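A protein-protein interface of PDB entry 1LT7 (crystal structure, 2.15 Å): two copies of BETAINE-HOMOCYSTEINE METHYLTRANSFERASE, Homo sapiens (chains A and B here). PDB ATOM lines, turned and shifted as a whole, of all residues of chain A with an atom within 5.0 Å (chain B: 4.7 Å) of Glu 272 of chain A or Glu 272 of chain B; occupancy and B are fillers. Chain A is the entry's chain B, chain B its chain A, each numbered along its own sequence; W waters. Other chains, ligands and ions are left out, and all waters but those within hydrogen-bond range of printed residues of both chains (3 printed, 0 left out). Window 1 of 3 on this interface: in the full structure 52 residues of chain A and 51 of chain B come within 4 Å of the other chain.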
ATOM      1  N   PHE A 269      -2.332 -16.173  20.705  1.00  0.00           N
ATOM      2  CA  PHE A 269      -3.505 -17.057  20.646  1.00  0.00           C
ATOM      3  C   PHE A 269      -3.625 -18.132  19.540  1.00  0.00           C
ATOM      4  O   PHE A 269      -4.704 -18.759  19.402  1.00  0.00           O
ATOM      5  CB  PHE A 269      -4.774 -16.187  20.603  1.00  0.00           C
ATOM      6  CG  PHE A 269      -4.842 -15.164  21.706  1.00  0.00           C
ATOM      7  CD1 PHE A 269      -4.970 -13.797  21.409  1.00  0.00           C
ATOM      8  CD2 PHE A 269      -4.800 -15.563  23.042  1.00  0.00           C
ATOM      9  CE1 PHE A 269      -5.063 -12.836  22.446  1.00  0.00           C
ATOM     10  CE2 PHE A 269      -4.893 -14.608  24.087  1.00  0.00           C
ATOM     11  CZ  PHE A 269      -5.026 -13.246  23.786  1.00  0.00           C
ATOM     12  N   GLY A 270      -2.551 -18.326  18.753  1.00  0.00           N
ATOM     13  CA  GLY A 270      -2.570 -19.336  17.704  1.00  0.00           C
ATOM     14  C   GLY A 270      -1.364 -20.282  17.770  1.00  0.00           C
ATOM     15  O   GLY A 270      -0.963 -20.896  16.755  1.00  0.00           O
ATOM     16  N   LEU A 271      -0.829 -20.424  18.980  1.00  0.00           N
ATOM     17  CA  LEU A 271       0.378 -21.212  19.234  1.00  0.00           C
ATOM     18  C   LEU A 271       0.199 -22.711  19.404  1.00  0.00           C
ATOM     19  O   LEU A 271       1.188 -23.435  19.390  1.00  0.00           O
ATOM     20  CB  LEU A 271       1.144 -20.660  20.473  1.00  0.00           C
ATOM     21  CG  LEU A 271       1.887 -19.300  20.384  1.00  0.00           C
ATOM     22  CD1 LEU A 271       2.810 -19.182  19.201  1.00  0.00           C
ATOM     23  CD2 LEU A 271       0.912 -18.238  20.333  1.00  0.00           C
ATOM     24  N   GLU A 272      -1.048 -23.170  19.554  1.00  0.00           N
ATOM     25  CA  GLU A 272      -1.307 -24.581  19.750  1.00  0.00           C
ATOM     26  C   GLU A 272      -0.529 -25.571  18.910  1.00  0.00           C
ATOM     27  O   GLU A 272       0.019 -26.535  19.443  1.00  0.00           O
ATOM     28  CB  GLU A 272      -2.796 -24.912  19.581  1.00  0.00           C
ATOM     29  CG  GLU A 272      -3.642 -24.637  20.813  1.00  0.00           C
ATOM     30  CD  GLU A 272      -4.030 -23.152  20.982  1.00  0.00           C
ATOM     31  OE1 GLU A 272      -4.887 -22.877  21.859  1.00  0.00           O
ATOM     32  OE2 GLU A 272      -3.503 -22.278  20.259  1.00  0.00           O
ATOM     33  N   PRO A 273      -0.494 -25.378  17.576  1.00  0.00           N
ATOM     34  CA  PRO A 273       0.235 -26.315  16.699  1.00  0.00           C
ATOM     35  C   PRO A 273       1.696 -26.557  17.070  1.00  0.00           C
ATOM     36  O   PRO A 273       2.243 -27.643  16.819  1.00  0.00           O
ATOM     37  CB  PRO A 273       0.155 -25.655  15.349  1.00  0.00           C
ATOM     38  CG  PRO A 273      -1.140 -24.805  15.461  1.00  0.00           C
ATOM     39  CD  PRO A 273      -1.035 -24.244  16.814  1.00  0.00           C
ATOM     40  N   ARG A 274       2.329 -25.539  17.653  1.00  0.00           N
ATOM     41  CA  ARG A 274       3.759 -25.606  17.985  1.00  0.00           C
ATOM     42  C   ARG A 274       4.077 -26.379  19.277  1.00  0.00           C
ATOM     43  O   ARG A 274       5.238 -26.677  19.566  1.00  0.00           O
ATOM     44  CB  ARG A 274       4.331 -24.153  18.102  1.00  0.00           C
ATOM     45  CG  ARG A 274       4.064 -23.231  16.842  1.00  0.00           C
ATOM     46  CD  ARG A 274       4.314 -21.721  17.112  1.00  0.00           C
ATOM     47  NE  ARG A 274       4.212 -20.948  15.867  1.00  0.00           N
ATOM     48  CZ  ARG A 274       5.224 -20.784  15.006  1.00  0.00           C
ATOM     49  NH1 ARG A 274       6.418 -21.325  15.270  1.00  0.00           N
ATOM     50  NH2 ARG A 274       5.044 -20.113  13.880  1.00  0.00           N
ATOM     51  N   VAL A 275       3.059 -26.677  20.067  1.00  0.00           N
ATOM     52  CA  VAL A 275       3.347 -27.335  21.329  1.00  0.00           C
ATOM     53  C   VAL A 275       4.140 -28.650  21.238  1.00  0.00           C
ATOM     54  O   VAL A 275       3.837 -29.535  20.439  1.00  0.00           O
ATOM     55  CB  VAL A 275       2.069 -27.538  22.156  1.00  0.00           C
ATOM     56  CG1 VAL A 275       2.416 -28.211  23.483  1.00  0.00           C
ATOM     57  CG2 VAL A 275       1.427 -26.153  22.435  1.00  0.00           C
ATOM     58  N   ALA A 276       5.182 -28.727  22.066  1.00  0.00           N
ATOM     59  CA  ALA A 276       6.053 -29.885  22.127  1.00  0.00           C
ATOM     60  C   ALA A 276       5.330 -31.134  22.657  1.00  0.00           C
ATOM     61  O   ALA A 276       4.475 -31.050  23.502  1.00  0.00           O
ATOM     62  CB  ALA A 276       7.264 -29.569  23.040  1.00  0.00           C
ATOM     63  N   THR A 277       5.640 -32.287  22.104  1.00  0.00           N
ATOM     64  CA  THR A 277       5.069 -33.504  22.639  1.00  0.00           C
ATOM     65  C   THR A 277       5.948 -33.886  23.854  1.00  0.00           C
ATOM     66  O   THR A 277       6.985 -33.258  24.144  1.00  0.00           O
ATOM     67  CB  THR A 277       5.196 -34.633  21.651  1.00  0.00           C
ATOM     68  OG1 THR A 277       6.573 -34.748  21.307  1.00  0.00           O
ATOM     69  CG2 THR A 277       4.339 -34.360  20.370  1.00  0.00           C
ATOM     70  N   ARG A 278       5.548 -34.921  24.565  1.00  0.00           N
ATOM     71  CA  ARG A 278       6.386 -35.327  25.668  1.00  0.00           C
ATOM     72  C   ARG A 278       7.745 -35.826  25.157  1.00  0.00           C
ATOM     73  O   ARG A 278       8.750 -35.652  25.855  1.00  0.00           O
ATOM     74  CB  ARG A 278       5.660 -36.364  26.533  1.00  0.00           C
ATOM     75  CG  ARG A 278       5.456 -37.713  25.957  1.00  0.00           C
ATOM     76  CD  ARG A 278       4.348 -38.367  26.773  1.00  0.00           C
ATOM     77  NE  ARG A 278       3.076 -37.737  26.426  1.00  0.00           N
ATOM     78  CZ  ARG A 278       1.947 -37.818  27.129  1.00  0.00           C
ATOM     79  NH1 ARG A 278       1.894 -38.512  28.271  1.00  0.00           N
ATOM     80  NH2 ARG A 278       0.862 -37.216  26.666  1.00  0.00           N
ATOM     81  N   TYR A 305       2.565 -32.266  32.432  1.00  0.00           N
ATOM     82  CA  TYR A 305       2.990 -33.445  31.713  1.00  0.00           C
ATOM     83  C   TYR A 305       4.326 -33.203  31.027  1.00  0.00           C
ATOM     84  O   TYR A 305       5.082 -34.138  30.841  1.00  0.00           O
ATOM     85  CB  TYR A 305       1.902 -33.958  30.745  1.00  0.00           C
ATOM     86  CG  TYR A 305       1.867 -33.320  29.350  1.00  0.00           C
ATOM     87  CD1 TYR A 305       1.307 -32.060  29.151  1.00  0.00           C
ATOM     88  CD2 TYR A 305       2.330 -34.031  28.215  1.00  0.00           C
ATOM     89  CE1 TYR A 305       1.193 -31.483  27.845  1.00  0.00           C
ATOM     90  CE2 TYR A 305       2.214 -33.482  26.901  1.00  0.00           C
ATOM     91  CZ  TYR A 305       1.651 -32.208  26.738  1.00  0.00           C
ATOM     92  OH  TYR A 305       1.570 -31.651  25.495  1.00  0.00           O
ATOM     93  N   PHE B 269      -0.108 -40.243  21.882  1.00  0.00           N
ATOM     94  CA  PHE B 269       0.931 -39.361  22.420  1.00  0.00           C
ATOM     95  C   PHE B 269       1.649 -38.371  21.491  1.00  0.00           C
ATOM     96  O   PHE B 269       2.666 -37.782  21.898  1.00  0.00           O
ATOM     97  CB  PHE B 269       1.984 -40.251  23.112  1.00  0.00           C
ATOM     98  CG  PHE B 269       1.407 -41.106  24.202  1.00  0.00           C
ATOM     99  CD1 PHE B 269       1.705 -42.461  24.283  1.00  0.00           C
ATOM    100  CD2 PHE B 269       0.537 -40.550  25.143  1.00  0.00           C
ATOM    101  CE1 PHE B 269       1.149 -43.274  25.288  1.00  0.00           C
ATOM    102  CE2 PHE B 269      -0.019 -41.351  26.144  1.00  0.00           C
ATOM    103  CZ  PHE B 269       0.303 -42.733  26.205  1.00  0.00           C
ATOM    104  N   GLY B 270       1.158 -38.196  20.259  1.00  0.00           N
ATOM    105  CA  GLY B 270       1.827 -37.256  19.376  1.00  0.00           C
ATOM    106  C   GLY B 270       0.839 -36.334  18.713  1.00  0.00           C
ATOM    107  O   GLY B 270       1.104 -35.813  17.627  1.00  0.00           O
ATOM    108  N   LEU B 271      -0.297 -36.131  19.389  1.00  0.00           N
ATOM    109  CA  LEU B 271      -1.414 -35.334  18.887  1.00  0.00           C
ATOM    110  C   LEU B 271      -1.343 -33.824  19.045  1.00  0.00           C
ATOM    111  O   LEU B 271      -2.169 -33.120  18.443  1.00  0.00           O
ATOM    112  CB  LEU B 271      -2.735 -35.834  19.526  1.00  0.00           C
ATOM    113  CG  LEU B 271      -3.053 -37.315  19.216  1.00  0.00           C
ATOM    114  CD1 LEU B 271      -4.262 -37.812  20.041  1.00  0.00           C
ATOM    115  CD2 LEU B 271      -3.336 -37.448  17.702  1.00  0.00           C
ATOM    116  N   GLU B 272      -0.391 -33.329  19.852  1.00  0.00           N
ATOM    117  CA  GLU B 272      -0.239 -31.882  20.071  1.00  0.00           C
ATOM    118  C   GLU B 272      -0.440 -30.939  18.878  1.00  0.00           C
ATOM    119  O   GLU B 272      -1.274 -30.055  18.935  1.00  0.00           O
ATOM    120  CB  GLU B 272       1.146 -31.563  20.683  1.00  0.00           C
ATOM    121  CG  GLU B 272       1.201 -31.864  22.197  1.00  0.00           C
ATOM    122  CD  GLU B 272       1.406 -33.364  22.557  1.00  0.00           C
ATOM    123  OE1 GLU B 272       1.259 -34.249  21.686  1.00  0.00           O
ATOM    124  OE2 GLU B 272       1.700 -33.655  23.733  1.00  0.00           O
ATOM    125  N   PRO B 273       0.286 -31.146  17.764  1.00  0.00           N
ATOM    126  CA  PRO B 273       0.125 -30.225  16.630  1.00  0.00           C
ATOM    127  C   PRO B 273      -1.302 -30.047  16.145  1.00  0.00           C
ATOM    128  O   PRO B 273      -1.659 -29.030  15.572  1.00  0.00           O
ATOM    129  CB  PRO B 273       0.988 -30.843  15.527  1.00  0.00           C
ATOM    130  CG  PRO B 273       1.861 -31.812  16.216  1.00  0.00           C
ATOM    131  CD  PRO B 273       1.094 -32.313  17.401  1.00  0.00           C
ATOM    132  N   ARG B 274      -2.125 -31.054  16.370  1.00  0.00           N
ATOM    133  CA  ARG B 274      -3.501 -31.024  15.859  1.00  0.00           C
ATOM    134  C   ARG B 274      -4.458 -30.237  16.730  1.00  0.00           C
ATOM    135  O   ARG B 274      -5.593 -29.956  16.321  1.00  0.00           O
ATOM    136  CB  ARG B 274      -4.004 -32.476  15.726  1.00  0.00           C
ATOM    137  CG  ARG B 274      -3.162 -33.400  14.788  1.00  0.00           C
ATOM    138  CD  ARG B 274      -3.546 -34.876  14.978  1.00  0.00           C
ATOM    139  NE  ARG B 274      -2.823 -35.756  14.047  1.00  0.00           N
ATOM    140  CZ  ARG B 274      -3.203 -35.999  12.785  1.00  0.00           C
ATOM    141  NH1 ARG B 274      -4.299 -35.451  12.286  1.00  0.00           N
ATOM    142  NH2 ARG B 274      -2.464 -36.761  12.010  1.00  0.00           N
ATOM    143  N   VAL B 275      -4.025 -29.897  17.941  1.00  0.00           N
ATOM    144  CA  VAL B 275      -4.938 -29.214  18.827  1.00  0.00           C
ATOM    145  C   VAL B 275      -5.584 -27.930  18.291  1.00  0.00           C
ATOM    146  O   VAL B 275      -4.931 -27.037  17.744  1.00  0.00           O
ATOM    147  CB  VAL B 275      -4.281 -28.977  20.218  1.00  0.00           C
ATOM    148  CG1 VAL B 275      -5.249 -28.278  21.148  1.00  0.00           C
ATOM    149  CG2 VAL B 275      -3.908 -30.333  20.858  1.00  0.00           C
ATOM    150  N   ALA B 276      -6.903 -27.867  18.452  1.00  0.00           N
ATOM    151  CA  ALA B 276      -7.703 -26.719  18.031  1.00  0.00           C
ATOM    152  C   ALA B 276      -7.317 -25.458  18.840  1.00  0.00           C
ATOM    153  O   ALA B 276      -7.058 -25.550  20.053  1.00  0.00           O
ATOM    154  CB  ALA B 276      -9.238 -27.036  18.282  1.00  0.00           C
ATOM    155  N   THR B 277      -7.271 -24.303  18.173  1.00  0.00           N
ATOM    156  CA  THR B 277      -7.051 -23.049  18.867  1.00  0.00           C
ATOM    157  C   THR B 277      -8.465 -22.628  19.353  1.00  0.00           C
ATOM    158  O   THR B 277      -9.501 -23.239  19.020  1.00  0.00           O
ATOM    159  CB  THR B 277      -6.599 -21.896  17.932  1.00  0.00           C
ATOM    160  OG1 THR B 277      -7.603 -21.708  16.914  1.00  0.00           O
ATOM    161  CG2 THR B 277      -5.198 -22.182  17.299  1.00  0.00           C
ATOM    162  N   ARG B 278      -8.514 -21.553  20.113  1.00  0.00           N
ATOM    163  CA  ARG B 278      -9.807 -21.107  20.528  1.00  0.00           C
ATOM    164  C   ARG B 278     -10.614 -20.585  19.324  1.00  0.00           C
ATOM    165  O   ARG B 278     -11.852 -20.660  19.342  1.00  0.00           O
ATOM    166  CB  ARG B 278      -9.674 -20.050  21.614  1.00  0.00           C
ATOM    167  CG  ARG B 278      -9.288 -18.742  21.157  1.00  0.00           C
ATOM    168  CD  ARG B 278      -8.955 -17.965  22.413  1.00  0.00           C
ATOM    169  NE  ARG B 278      -7.664 -18.400  22.931  1.00  0.00           N
ATOM    170  CZ  ARG B 278      -7.312 -18.386  24.214  1.00  0.00           C
ATOM    171  NH1 ARG B 278      -6.092 -18.796  24.572  1.00  0.00           N
ATOM    172  NH2 ARG B 278      -8.188 -17.982  25.130  1.00  0.00           N
ATOM    173  N   TYR B 305     -10.235 -24.124  28.500  1.00  0.00           N
ATOM    174  CA  TYR B 305     -10.220 -22.909  27.675  1.00  0.00           C
ATOM    175  C   TYR B 305     -10.976 -23.105  26.366  1.00  0.00           C
ATOM    176  O   TYR B 305     -11.555 -22.168  25.861  1.00  0.00           O
ATOM    177  CB  TYR B 305      -8.781 -22.366  27.475  1.00  0.00           C
ATOM    178  CG  TYR B 305      -7.974 -23.030  26.370  1.00  0.00           C
ATOM    179  CD1 TYR B 305      -7.780 -22.394  25.143  1.00  0.00           C
ATOM    180  CD2 TYR B 305      -7.401 -24.276  26.562  1.00  0.00           C
ATOM    181  CE1 TYR B 305      -7.027 -22.992  24.116  1.00  0.00           C
ATOM    182  CE2 TYR B 305      -6.626 -24.901  25.535  1.00  0.00           C
ATOM    183  CZ  TYR B 305      -6.453 -24.255  24.329  1.00  0.00           C
ATOM    184  OH  TYR B 305      -5.718 -24.861  23.340  1.00  0.00           O
HETATM  185  O   HOH W   1      -1.204 -28.408  21.076  1.00  0.00           O
HETATM  186  O   HOH W   2      -6.058 -20.483  21.261  1.00  0.00           O
HETATM  187  O   HOH W   3       2.862 -35.968  24.163  1.00  0.00           O
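Water W3 lies within hydrogen-bond range of the side-chain carboxylate (OE2) of Glu 272 of chain B (2.6 Å), the guanidinium group (NE) of Arg 278 of chain A (2.9 Å) and the backbone carbonyl oxygen (O) of Phe 269 of chain B (2.9 Å). Water W1 bridges O of Glu 272 of chain B (2.7 Å) and O of Glu 272 of chain A (2.8 Å). Water W2 lies within hydrogen-bond range of the side-chain carboxylate (OE1) of Glu 272 of chain A (2.7 Å), the backbone carbonyl oxygen (O) of Phe 269 of chain A (2.9 Å) and the backbone NH (N) of Arg 278 of chain B (2.9 Å).
Printed residues of chain A that touch a printed residue of chain B: Phe 269, Gly 270, Glu 272, Pro 273, Val 275, Ala 276, Thr 277, Arg 278 and Tyr 305. Hydrophobic or aromatic side chains of chain A within 4 Å of the printed part of chain B: Phe 269, Pro 273 and Tyr 305. Among the printed residues, 15 pairs touch across the chains.
Phe 269 of chain A touches Thr 277 of chain B, but with the chains exchanged Thr 277 of chain A does not touch Phe 269 of chain B (4.05 Å). Phe 269 of chain A touches Arg 278 of chain B, and with the chains exchanged Arg 278 of chain A touches Phe 269 of chain B. Glu 272 of chain B touches its own counterpart, Glu 272 of chain A. Glu 272 of chain A touches Tyr 305 of chain B, and with the chains exchanged Tyr 305 of chain A touches Glu 272 of chain B. Of the 15 pairs that touch across the chains among the printed residues, 14 have their exchanged pair printed and touching as well.
Among the printed residues, pairs that only touch across the chains: Phe 269 of chain A with Thr 277 of chain B (3.9 Å), Phe 269 of chain A with Arg 278 of chain B (3.8 Å), Gly 270 of chain A with Thr 277 of chain B (3.9 Å), Glu 272 of chain A with Glu 272 of chain B (3.8 Å), Glu 272 of chain A with Val 275 of chain B (3.5 Å), Glu 272 of chain A with Ala 276 of chain B (3.6 Å), Glu 272 of chain A with Thr 277 of chain B (3.4 Å), Pro 273 of chain A with Pro 273 of chain B (3.3 Å), Val 275 of chain A with Glu 272 of chain B (3.4 Å), Ala 276 of chain A with Glu 272 of chain B (3.6 Å), Thr 277 of chain A with Gly 270 of chain B (3.96 Å), Thr 277 of chain A with Glu 272 of chain B (3.4 Å) and Arg 278 of chain A with Phe 269 of chain B (3.7 Å).
OE2 of Glu 272 of chain B lies within hydrogen-bond range of OH of Tyr 305 of chain A (2.7 Å). The side-chain carboxylate (OE1) of Glu 272 of chain A lies within hydrogen-bond range of the side-chain hydroxyl (OH) of Tyr 305 of chain B (2.6 Å).
Printed residues of chain B within 4 Å of Gly 270 of chain A: Thr 277. Leu 271 of chain A touches none of the printed residues of chain B. Of the printed residues of chain B, Pro 273 of chain A touches Pro 273 (3.3 Å). Printed residues of chain A within 4 Å of Arg 278 of chain B: Phe 269. The nearest residue of chain B that does not touch Glu 272 of chain A is Arg 278 of chain B (4.2 Å). The nearest residue of chain A that does not touch Glu 272 of chain B is Arg 278 of chain A (4.1 Å). The nearest printed residue of chain B that does not touch Tyr 305 of chain A is Phe 269 of chain B (6.6 Å).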
